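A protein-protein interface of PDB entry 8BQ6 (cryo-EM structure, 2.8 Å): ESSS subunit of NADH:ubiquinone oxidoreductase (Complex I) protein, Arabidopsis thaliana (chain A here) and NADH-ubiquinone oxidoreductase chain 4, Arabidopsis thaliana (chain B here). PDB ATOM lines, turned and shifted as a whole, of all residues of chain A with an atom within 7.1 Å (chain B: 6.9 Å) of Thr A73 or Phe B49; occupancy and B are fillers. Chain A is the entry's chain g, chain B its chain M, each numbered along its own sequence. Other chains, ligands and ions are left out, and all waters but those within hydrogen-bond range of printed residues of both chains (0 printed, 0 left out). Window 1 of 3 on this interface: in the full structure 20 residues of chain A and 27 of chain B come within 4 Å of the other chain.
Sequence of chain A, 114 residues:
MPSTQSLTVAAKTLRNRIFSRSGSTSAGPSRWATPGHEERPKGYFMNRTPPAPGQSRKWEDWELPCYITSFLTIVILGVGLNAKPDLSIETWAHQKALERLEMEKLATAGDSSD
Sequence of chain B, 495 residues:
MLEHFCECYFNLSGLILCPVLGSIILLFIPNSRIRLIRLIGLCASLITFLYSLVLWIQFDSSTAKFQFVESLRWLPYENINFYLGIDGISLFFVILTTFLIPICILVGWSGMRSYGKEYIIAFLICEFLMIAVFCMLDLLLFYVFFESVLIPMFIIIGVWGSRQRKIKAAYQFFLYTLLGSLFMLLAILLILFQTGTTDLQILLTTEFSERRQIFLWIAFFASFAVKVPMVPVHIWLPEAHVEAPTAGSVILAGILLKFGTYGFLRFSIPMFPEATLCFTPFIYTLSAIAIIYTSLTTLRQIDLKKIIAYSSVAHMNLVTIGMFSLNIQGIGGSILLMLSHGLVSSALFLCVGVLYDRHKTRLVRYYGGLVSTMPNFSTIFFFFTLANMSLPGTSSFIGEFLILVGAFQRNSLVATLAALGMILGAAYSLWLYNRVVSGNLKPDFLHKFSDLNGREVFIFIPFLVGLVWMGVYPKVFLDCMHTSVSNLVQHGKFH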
ATOM      1  N   CYS A  66       1.668  13.312  26.437  1.00  0.00           N
ATOM      2  CA  CYS A  66       2.078  12.675  25.193  1.00  0.00           C
ATOM      3  C   CYS A  66       1.654  13.489  23.978  1.00  0.00           C
ATOM      4  O   CYS A  66       2.402  13.576  22.997  1.00  0.00           O
ATOM      5  CB  CYS A  66       1.520  11.256  25.127  1.00  0.00           C
ATOM      6  SG  CYS A  66       2.514  10.067  26.052  1.00  0.00           S
ATOM      7  N   ILE A  68       1.308  16.663  23.915  1.00  0.00           N
ATOM      8  CA  ILE A  68       2.121  17.871  23.896  1.00  0.00           C
ATOM      9  C   ILE A  68       3.523  17.551  23.407  1.00  0.00           C
ATOM     10  O   ILE A  68       4.141  18.339  22.680  1.00  0.00           O
ATOM     11  CB  ILE A  68       2.129  18.520  25.288  1.00  0.00           C
ATOM     12  CG1 ILE A  68       0.791  19.215  25.537  1.00  0.00           C
ATOM     13  CG2 ILE A  68       3.295  19.482  25.437  1.00  0.00           C
ATOM     14  CD1 ILE A  68       0.660  19.807  26.906  1.00  0.00           C
ATOM     15  N   THR A  69       4.047  16.390  23.797  1.00  0.00           N
ATOM     16  CA  THR A  69       5.336  15.955  23.279  1.00  0.00           C
ATOM     17  C   THR A  69       5.254  15.695  21.781  1.00  0.00           C
ATOM     18  O   THR A  69       6.169  16.050  21.029  1.00  0.00           O
ATOM     19  CB  THR A  69       5.801  14.706  24.024  1.00  0.00           C
ATOM     20  OG1 THR A  69       6.014  15.029  25.403  1.00  0.00           O
ATOM     21  CG2 THR A  69       7.102  14.207  23.444  1.00  0.00           C
ATOM     22  N   SER A  70       4.156  15.084  21.330  1.00  0.00           N
ATOM     23  CA  SER A  70       3.965  14.832  19.905  1.00  0.00           C
ATOM     24  C   SER A  70       3.875  16.130  19.118  1.00  0.00           C
ATOM     25  O   SER A  70       4.405  16.227  18.006  1.00  0.00           O
ATOM     26  CB  SER A  70       2.708  13.996  19.682  1.00  0.00           C
ATOM     27  OG  SER A  70       2.912  12.654  20.080  1.00  0.00           O
ATOM     28  N   PHE A  71       3.182  17.127  19.665  1.00  0.00           N
ATOM     29  CA  PHE A  71       3.074  18.408  18.978  1.00  0.00           C
ATOM     30  C   PHE A  71       4.421  19.116  18.921  1.00  0.00           C
ATOM     31  O   PHE A  71       4.816  19.634  17.870  1.00  0.00           O
ATOM     32  CB  PHE A  71       2.030  19.278  19.671  1.00  0.00           C
ATOM     33  CG  PHE A  71       2.035  20.698  19.215  1.00  0.00           C
ATOM     34  CD1 PHE A  71       1.508  21.038  17.984  1.00  0.00           C
ATOM     35  CD2 PHE A  71       2.552  21.696  20.020  1.00  0.00           C
ATOM     36  CE1 PHE A  71       1.509  22.344  17.557  1.00  0.00           C
ATOM     37  CE2 PHE A  71       2.552  23.004  19.599  1.00  0.00           C
ATOM     38  CZ  PHE A  71       2.030  23.330  18.364  1.00  0.00           C
ATOM     39  N   LEU A  72       5.144  19.137  20.041  1.00  0.00           N
ATOM     40  CA  LEU A  72       6.446  19.793  20.084  1.00  0.00           C
ATOM     41  C   LEU A  72       7.465  19.067  19.212  1.00  0.00           C
ATOM     42  O   LEU A  72       8.400  19.687  18.694  1.00  0.00           O
ATOM     43  CB  LEU A  72       6.933  19.873  21.529  1.00  0.00           C
ATOM     44  CG  LEU A  72       6.171  20.809  22.471  1.00  0.00           C
ATOM     45  CD1 LEU A  72       6.833  20.840  23.836  1.00  0.00           C
ATOM     46  CD2 LEU A  72       6.098  22.206  21.888  1.00  0.00           C
ATOM     47  N   THR A  73       7.306  17.750  19.051  1.00  0.00           N
ATOM     48  CA  THR A  73       8.225  16.979  18.217  1.00  0.00           C
ATOM     49  C   THR A  73       8.133  17.401  16.756  1.00  0.00           C
ATOM     50  O   THR A  73       9.156  17.576  16.084  1.00  0.00           O
ATOM     51  CB  THR A  73       7.928  15.484  18.363  1.00  0.00           C
ATOM     52  OG1 THR A  73       8.292  15.050  19.678  1.00  0.00           O
ATOM     53  CG2 THR A  73       8.707  14.672  17.339  1.00  0.00           C
ATOM     54  N   ILE A  74       6.911  17.565  16.245  1.00  0.00           N
ATOM     55  CA  ILE A  74       6.732  17.979  14.855  1.00  0.00           C
ATOM     56  C   ILE A  74       7.196  19.416  14.665  1.00  0.00           C
ATOM     57  O   ILE A  74       7.765  19.773  13.629  1.00  0.00           O
ATOM     58  CB  ILE A  74       5.268  17.803  14.415  1.00  0.00           C
ATOM     59  CG1 ILE A  74       4.715  16.457  14.880  1.00  0.00           C
ATOM     60  CG2 ILE A  74       5.158  17.902  12.905  1.00  0.00           C
ATOM     61  CD1 ILE A  74       5.350  15.269  14.206  1.00  0.00           C
ATOM     62  N   VAL A  75       6.946  20.268  15.660  1.00  0.00           N
ATOM     63  CA  VAL A  75       7.305  21.677  15.532  1.00  0.00           C
ATOM     64  C   VAL A  75       8.820  21.849  15.546  1.00  0.00           C
ATOM     65  O   VAL A  75       9.379  22.605  14.744  1.00  0.00           O
ATOM     66  CB  VAL A  75       6.622  22.508  16.632  1.00  0.00           C
ATOM     67  CG1 VAL A  75       7.288  23.866  16.757  1.00  0.00           C
ATOM     68  CG2 VAL A  75       5.141  22.665  16.318  1.00  0.00           C
ATOM     69  N   ILE A  76       9.509  21.146  16.444  1.00  0.00           N
ATOM     70  CA  ILE A  76      10.965  21.264  16.506  1.00  0.00           C
ATOM     71  C   ILE A  76      11.604  20.693  15.245  1.00  0.00           C
ATOM     72  O   ILE A  76      12.467  21.324  14.625  1.00  0.00           O
ATOM     73  CB  ILE A  76      11.511  20.583  17.773  1.00  0.00           C
ATOM     74  CG1 ILE A  76      11.309  21.487  18.984  1.00  0.00           C
ATOM     75  CG2 ILE A  76      12.983  20.265  17.617  1.00  0.00           C
ATOM     76  CD1 ILE A  76      11.486  20.773  20.296  1.00  0.00           C
ATOM     77  N   LEU A  77      11.189  19.492  14.844  1.00  0.00           N
ATOM     78  CA  LEU A  77      11.798  18.848  13.684  1.00  0.00           C
ATOM     79  C   LEU A  77      11.293  19.459  12.379  1.00  0.00           C
ATOM     80  O   LEU A  77      12.035  19.545  11.395  1.00  0.00           O
ATOM     81  CB  LEU A  77      11.520  17.347  13.715  1.00  0.00           C
ATOM     82  CG  LEU A  77      12.200  16.536  14.820  1.00  0.00           C
ATOM     83  CD1 LEU A  77      11.860  15.062  14.678  1.00  0.00           C
ATOM     84  CD2 LEU A  77      13.705  16.750  14.815  1.00  0.00           C
ATOM     85  N   GLY A  78      10.023  19.865  12.344  1.00  0.00           N
ATOM     86  CA  GLY A  78       9.493  20.485  11.140  1.00  0.00           C
ATOM     87  C   GLY A  78      10.090  21.850  10.863  1.00  0.00           C
ATOM     88  O   GLY A  78      10.325  22.207   9.706  1.00  0.00           O
ATOM     89  N   VAL A  79      10.335  22.628  11.912  1.00  0.00           N
ATOM     90  CA  VAL A  79      10.932  23.950  11.771  1.00  0.00           C
ATOM     91  C   VAL A  79      12.449  23.881  11.854  1.00  0.00           C
ATOM     92  O   VAL A  79      13.152  24.418  10.995  1.00  0.00           O
ATOM     93  CB  VAL A  79      10.350  24.903  12.840  1.00  0.00           C
ATOM     94  CG1 VAL A  79      11.342  26.008  13.191  1.00  0.00           C
ATOM     95  CG2 VAL A  79       9.033  25.483  12.374  1.00  0.00           C
ATOM     96  N   LEU B  15      21.356  16.772  29.654  1.00  0.00           N
ATOM     97  CA  LEU B  15      20.694  15.560  29.185  1.00  0.00           C
ATOM     98  C   LEU B  15      21.013  14.363  30.066  1.00  0.00           C
ATOM     99  O   LEU B  15      20.121  13.563  30.367  1.00  0.00           O
ATOM    100  CB  LEU B  15      21.087  15.276  27.738  1.00  0.00           C
ATOM    101  CG  LEU B  15      20.320  14.154  27.048  1.00  0.00           C
ATOM    102  CD1 LEU B  15      19.023  14.656  26.468  1.00  0.00           C
ATOM    103  CD2 LEU B  15      21.191  13.592  25.948  1.00  0.00           C
ATOM    104  N   CYS B  43       6.957  12.334  32.394  1.00  0.00           N
ATOM    105  CA  CYS B  43       7.364  13.688  32.041  1.00  0.00           C
ATOM    106  C   CYS B  43       8.878  13.824  31.985  1.00  0.00           C
ATOM    107  O   CYS B  43       9.407  14.502  31.096  1.00  0.00           O
ATOM    108  CB  CYS B  43       6.769  14.687  33.028  1.00  0.00           C
ATOM    109  SG  CYS B  43       5.071  15.128  32.635  1.00  0.00           S
ATOM    110  N   ALA B  44       9.595  13.204  32.925  1.00  0.00           N
ATOM    111  CA  ALA B  44      11.052  13.263  32.886  1.00  0.00           C
ATOM    112  C   ALA B  44      11.581  12.648  31.598  1.00  0.00           C
ATOM    113  O   ALA B  44      12.432  13.236  30.911  1.00  0.00           O
ATOM    114  CB  ALA B  44      11.638  12.554  34.107  1.00  0.00           C
ATOM    115  N   SER B  45      11.057  11.473  31.233  1.00  0.00           N
ATOM    116  CA  SER B  45      11.497  10.836  29.994  1.00  0.00           C
ATOM    117  C   SER B  45      11.155  11.685  28.769  1.00  0.00           C
ATOM    118  O   SER B  45      11.965  11.799  27.836  1.00  0.00           O
ATOM    119  CB  SER B  45      10.891   9.440  29.887  1.00  0.00           C
ATOM    120  OG  SER B  45       9.491   9.479  30.082  1.00  0.00           O
ATOM    121  N   LEU B  46       9.968  12.297  28.749  1.00  0.00           N
ATOM    122  CA  LEU B  46       9.581  13.089  27.584  1.00  0.00           C
ATOM    123  C   LEU B  46      10.430  14.351  27.451  1.00  0.00           C
ATOM    124  O   LEU B  46      10.778  14.760  26.333  1.00  0.00           O
ATOM    125  CB  LEU B  46       8.100  13.450  27.654  1.00  0.00           C
ATOM    126  CG  LEU B  46       7.106  12.298  27.511  1.00  0.00           C
ATOM    127  CD1 LEU B  46       5.705  12.783  27.836  1.00  0.00           C
ATOM    128  CD2 LEU B  46       7.160  11.667  26.129  1.00  0.00           C
ATOM    129  N   ILE B  47      10.767  14.988  28.574  1.00  0.00           N
ATOM    130  CA  ILE B  47      11.626  16.165  28.511  1.00  0.00           C
ATOM    131  C   ILE B  47      13.016  15.773  28.035  1.00  0.00           C
ATOM    132  O   ILE B  47      13.664  16.517  27.290  1.00  0.00           O
ATOM    133  CB  ILE B  47      11.669  16.884  29.870  1.00  0.00           C
ATOM    134  CG1 ILE B  47      10.305  17.497  30.170  1.00  0.00           C
ATOM    135  CG2 ILE B  47      12.720  17.985  29.865  1.00  0.00           C
ATOM    136  CD1 ILE B  47      10.044  17.691  31.625  1.00  0.00           C
ATOM    137  N   THR B  48      13.493  14.596  28.444  1.00  0.00           N
ATOM    138  CA  THR B  48      14.770  14.122  27.922  1.00  0.00           C
ATOM    139  C   THR B  48      14.711  13.918  26.408  1.00  0.00           C
ATOM    140  O   THR B  48      15.652  14.280  25.686  1.00  0.00           O
ATOM    141  CB  THR B  48      15.174  12.835  28.638  1.00  0.00           C
ATOM    142  OG1 THR B  48      14.947  12.990  30.044  1.00  0.00           O
ATOM    143  CG2 THR B  48      16.642  12.536  28.408  1.00  0.00           C
ATOM    144  N   PHE B  49      13.604  13.357  25.907  1.00  0.00           N
ATOM    145  CA  PHE B  49      13.451  13.190  24.461  1.00  0.00           C
ATOM    146  C   PHE B  49      13.486  14.534  23.733  1.00  0.00           C
ATOM    147  O   PHE B  49      14.162  14.679  22.702  1.00  0.00           O
ATOM    148  CB  PHE B  49      12.147  12.449  24.154  1.00  0.00           C
ATOM    149  CG  PHE B  49      11.873  12.276  22.685  1.00  0.00           C
ATOM    150  CD1 PHE B  49      12.797  11.665  21.858  1.00  0.00           C
ATOM    151  CD2 PHE B  49      10.684  12.723  22.134  1.00  0.00           C
ATOM    152  CE1 PHE B  49      12.544  11.507  20.510  1.00  0.00           C
ATOM    153  CE2 PHE B  49      10.427  12.566  20.788  1.00  0.00           C
ATOM    154  CZ  PHE B  49      11.358  11.957  19.975  1.00  0.00           C
ATOM    155  N   LEU B  50      12.768  15.531  24.257  1.00  0.00           N
ATOM    156  CA  LEU B  50      12.764  16.848  23.621  1.00  0.00           C
ATOM    157  C   LEU B  50      14.148  17.492  23.656  1.00  0.00           C
ATOM    158  O   LEU B  50      14.586  18.119  22.679  1.00  0.00           O
ATOM    159  CB  LEU B  50      11.741  17.752  24.299  1.00  0.00           C
ATOM    160  CG  LEU B  50      10.296  17.273  24.195  1.00  0.00           C
ATOM    161  CD1 LEU B  50       9.404  18.123  25.081  1.00  0.00           C
ATOM    162  CD2 LEU B  50       9.821  17.296  22.752  1.00  0.00           C
ATOM    163  N   TYR B  51      14.845  17.353  24.783  1.00  0.00           N
ATOM    164  CA  TYR B  51      16.200  17.876  24.910  1.00  0.00           C
ATOM    165  C   TYR B  51      17.125  17.274  23.854  1.00  0.00           C
ATOM    166  O   TYR B  51      17.909  17.991  23.210  1.00  0.00           O
ATOM    167  CB  TYR B  51      16.686  17.587  26.332  1.00  0.00           C
ATOM    168  CG  TYR B  51      17.863  18.387  26.815  1.00  0.00           C
ATOM    169  CD1 TYR B  51      19.104  18.232  26.235  1.00  0.00           C
ATOM    170  CD2 TYR B  51      17.735  19.290  27.859  1.00  0.00           C
ATOM    171  CE1 TYR B  51      20.185  18.942  26.676  1.00  0.00           C
ATOM    172  CE2 TYR B  51      18.817  20.016  28.305  1.00  0.00           C
ATOM    173  CZ  TYR B  51      20.041  19.834  27.704  1.00  0.00           C
ATOM    174  OH  TYR B  51      21.136  20.542  28.131  1.00  0.00           O
ATOM    175  N   SER B  52      17.035  15.958  23.647  1.00  0.00           N
ATOM    176  CA  SER B  52      17.852  15.312  22.621  1.00  0.00           C
ATOM    177  C   SER B  52      17.483  15.796  21.222  1.00  0.00           C
ATOM    178  O   SER B  52      18.351  15.912  20.344  1.00  0.00           O
ATOM    179  CB  SER B  52      17.700  13.799  22.702  1.00  0.00           C
ATOM    180  OG  SER B  52      16.577  13.381  21.949  1.00  0.00           O
ATOM    181  N   LEU B  53      16.195  16.047  20.981  1.00  0.00           N
ATOM    182  CA  LEU B  53      15.806  16.611  19.693  1.00  0.00           C
ATOM    183  C   LEU B  53      16.471  17.966  19.470  1.00  0.00           C
ATOM    184  O   LEU B  53      16.909  18.285  18.354  1.00  0.00           O
ATOM    185  CB  LEU B  53      14.288  16.743  19.617  1.00  0.00           C
ATOM    186  CG  LEU B  53      13.463  15.470  19.440  1.00  0.00           C
ATOM    187  CD1 LEU B  53      12.070  15.853  18.986  1.00  0.00           C
ATOM    188  CD2 LEU B  53      14.110  14.503  18.460  1.00  0.00           C
ATOM    189  N   VAL B  54      16.557  18.777  20.525  1.00  0.00           N
ATOM    190  CA  VAL B  54      17.231  20.067  20.390  1.00  0.00           C
ATOM    191  C   VAL B  54      18.707  19.867  20.056  1.00  0.00           C
ATOM    192  O   VAL B  54      19.260  20.557  19.190  1.00  0.00           O
ATOM    193  CB  VAL B  54      17.032  20.920  21.655  1.00  0.00           C
ATOM    194  CG1 VAL B  54      17.806  22.214  21.534  1.00  0.00           C
ATOM    195  CG2 VAL B  54      15.553  21.224  21.851  1.00  0.00           C
ATOM    196  N   VAL B  94      21.920   8.354  20.810  1.00  0.00           N
ATOM    197  CA  VAL B  94      21.403   9.126  21.936  1.00  0.00           C
ATOM    198  C   VAL B  94      19.927   9.433  21.732  1.00  0.00           C
ATOM    199  O   VAL B  94      19.103   9.283  22.649  1.00  0.00           O
ATOM    200  CB  VAL B  94      22.223  10.413  22.119  1.00  0.00           C
ATOM    201  CG1 VAL B  94      21.862  11.079  23.409  1.00  0.00           C
ATOM    202  CG2 VAL B  94      23.697  10.086  22.129  1.00  0.00           C
ATOM    203  N   ILE B  95      19.569   9.868  20.521  1.00  0.00           N
ATOM    204  CA  ILE B  95      18.170  10.179  20.241  1.00  0.00           C
ATOM    205  C   ILE B  95      17.300   8.937  20.415  1.00  0.00           C
ATOM    206  O   ILE B  95      16.216   8.993  21.010  1.00  0.00           O
ATOM    207  CB  ILE B  95      18.033  10.774  18.830  1.00  0.00           C
ATOM    208  CG1 ILE B  95      18.411  12.250  18.843  1.00  0.00           C
ATOM    209  CG2 ILE B  95      16.615  10.635  18.325  1.00  0.00           C
ATOM    210  CD1 ILE B  95      18.638  12.805  17.470  1.00  0.00           C
ATOM    211  N   LEU B  96      17.769   7.798  19.900  1.00  0.00           N
ATOM    212  CA  LEU B  96      17.012   6.554  19.973  1.00  0.00           C
ATOM    213  C   LEU B  96      16.796   6.110  21.412  1.00  0.00           C
ATOM    214  O   LEU B  96      15.712   5.632  21.763  1.00  0.00           O
ATOM    215  CB  LEU B  96      17.732   5.463  19.184  1.00  0.00           C
ATOM    216  CG  LEU B  96      16.922   4.179  19.015  1.00  0.00           C
ATOM    217  CD1 LEU B  96      15.724   4.416  18.117  1.00  0.00           C
ATOM    218  CD2 LEU B  96      17.795   3.062  18.480  1.00  0.00           C
ATOM    219  N   THR B  97      17.821   6.241  22.255  1.00  0.00           N
ATOM    220  CA  THR B  97      17.648   5.930  23.672  1.00  0.00           C
ATOM    221  C   THR B  97      16.587   6.824  24.304  1.00  0.00           C
ATOM    222  O   THR B  97      15.656   6.342  24.986  1.00  0.00           O
ATOM    223  CB  THR B  97      18.984   6.093  24.398  1.00  0.00           C
ATOM    224  OG1 THR B  97      19.934   5.166  23.862  1.00  0.00           O
ATOM    225  CG2 THR B  97      18.824   5.859  25.891  1.00  0.00           C
ATOM    226  N   THR B  98      16.715   8.139  24.088  1.00  0.00           N
ATOM    227  CA  THR B  98      15.790   9.076  24.710  1.00  0.00           C
ATOM    228  C   THR B  98      14.375   8.861  24.209  1.00  0.00           C
ATOM    229  O   THR B  98      13.412   9.203  24.900  1.00  0.00           O
ATOM    230  CB  THR B  98      16.217  10.519  24.446  1.00  0.00           C
ATOM    231  OG1 THR B  98      16.430  10.713  23.044  1.00  0.00           O
ATOM    232  CG2 THR B  98      17.508  10.808  25.168  1.00  0.00           C
ATOM    233  N   PHE B  99      14.230   8.305  23.010  1.00  0.00           N
ATOM    234  CA  PHE B  99      12.895   8.055  22.487  1.00  0.00           C
ATOM    235  C   PHE B  99      12.319   6.745  23.007  1.00  0.00           C
ATOM    236  O   PHE B  99      11.115   6.658  23.268  1.00  0.00           O
ATOM    237  CB  PHE B  99      12.918   8.048  20.964  1.00  0.00           C
ATOM    238  CG  PHE B  99      11.751   7.350  20.365  1.00  0.00           C
ATOM    239  CD1 PHE B  99      10.494   7.917  20.430  1.00  0.00           C
ATOM    240  CD2 PHE B  99      11.899   6.122  19.754  1.00  0.00           C
ATOM    241  CE1 PHE B  99       9.410   7.275  19.894  1.00  0.00           C
ATOM    242  CE2 PHE B  99      10.817   5.479  19.212  1.00  0.00           C
ATOM    243  CZ  PHE B  99       9.571   6.054  19.281  1.00  0.00           C
ATOM    244  N   LEU B 100      13.154   5.716  23.156  1.00  0.00           N
ATOM    245  CA  LEU B 100      12.630   4.414  23.550  1.00  0.00           C
ATOM    246  C   LEU B 100      12.220   4.367  25.011  1.00  0.00           C
ATOM    247  O   LEU B 100      11.334   3.583  25.370  1.00  0.00           O
ATOM    248  CB  LEU B 100      13.652   3.320  23.283  1.00  0.00           C
ATOM    249  CG  LEU B 100      13.711   2.865  21.837  1.00  0.00           C
ATOM    250  CD1 LEU B 100      14.670   1.710  21.743  1.00  0.00           C
ATOM    251  CD2 LEU B 100      12.322   2.465  21.380  1.00  0.00           C
ATOM    252  N   PRO B 102      10.552   6.591  27.077  1.00  0.00           N
ATOM    253  CA  PRO B 102       9.129   6.887  27.323  1.00  0.00           C
ATOM    254  C   PRO B 102       8.196   5.810  26.810  1.00  0.00           C
ATOM    255  O   PRO B 102       7.132   5.589  27.400  1.00  0.00           O
ATOM    256  CB  PRO B 102       8.909   8.216  26.588  1.00  0.00           C
ATOM    257  CG  PRO B 102      10.242   8.788  26.405  1.00  0.00           C
ATOM    258  CD  PRO B 102      11.199   7.660  26.303  1.00  0.00           C
ATOM    259  N   GLU B 127      18.330   4.655  31.424  1.00  0.00           N
ATOM    260  CA  GLU B 127      18.421   5.781  30.454  1.00  0.00           C
ATOM    261  C   GLU B 127      19.696   6.583  30.706  1.00  0.00           C
ATOM    262  O   GLU B 127      20.438   6.795  29.738  1.00  0.00           O
ATOM    263  CB  GLU B 127      17.197   6.693  30.560  1.00  0.00           C
ATOM    264  CG  GLU B 127      17.259   7.921  29.671  1.00  0.00           C
ATOM    265  CD  GLU B 127      15.946   8.643  29.427  1.00  0.00           C
ATOM    266  OE1 GLU B 127      15.264   8.982  30.409  1.00  0.00           O
ATOM    267  OE2 GLU B 127      15.611   8.872  28.253  1.00  0.00           O
ATOM    268  N   PRO B 462       4.645   6.651  16.683  1.00  0.00           N
ATOM    269  CA  PRO B 462       6.001   7.113  16.335  1.00  0.00           C
ATOM    270  C   PRO B 462       6.858   6.041  15.688  1.00  0.00           C
ATOM    271  O   PRO B 462       7.830   6.375  15.002  1.00  0.00           O
ATOM    272  CB  PRO B 462       6.595   7.576  17.674  1.00  0.00           C
ATOM    273  CG  PRO B 462       5.645   7.224  18.718  1.00  0.00           C
ATOM    274  CD  PRO B 462       4.395   6.680  18.136  1.00  0.00           C
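O of Phe B49 sits at hydrogen-bond distance from OG of Ser B52 (2.8 Å).
The side-chain hydroxyl (OG1) of Thr A73 sits at hydrogen-bond distance from the backbone carbonyl oxygen (O) of Thr A69 (2.7 Å).
Thr A69 touches Leu B46 (OG1 to CD1, 3.3 Å).
Leu A72 touches Leu B50 (CD1 to CD1, 3.9 Å).
OG1 of Thr A73 touches CE2 of Phe B49 (3.5 Å).
Thr A73 touches Leu B53.
Of chain B, only Phe B49 (3.5 Å) and Leu B53 (3.9 Å) come within 4 Å of Thr A73.
Printed residues of chain A within 4 Å of Phe B49: Thr A73 (3.5 Å).
Printed residues of chain B within 4 Å of Thr A69: Leu B46 (3.3 Å).
Printed residues of chain A within 4 Å of Leu B53: Thr A73 (3.9 Å).
Printed residues of chain A within 4 Å of Leu B50: Leu A72.
Printed residues of chain B within 4 Å of Leu A72: Leu B50 (3.9 Å).
The nearest residue of chain A that does not touch Phe B49 is Thr A69 (4.1 Å).
The nearest printed residue of chain A that does not touch Leu B50 is Thr A73 (4.1 Å).
Of the 23 printed residues of chain B, 4 touch a printed residue of chain A.
Hydrophobic or aromatic side chains of chain B within 4 Å of the printed part of chain A: Leu B46, Phe B49, Leu B50 and Leu B53.
Printed residues of chain A that touch a printed residue of chain B: Thr A69, Leu A72 and Thr A73.
Hydrophobic or aromatic side chains of chain A that line the printed part of chain B: Leu A72.
Among the printed residues, 4 pairs touch across the chains.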
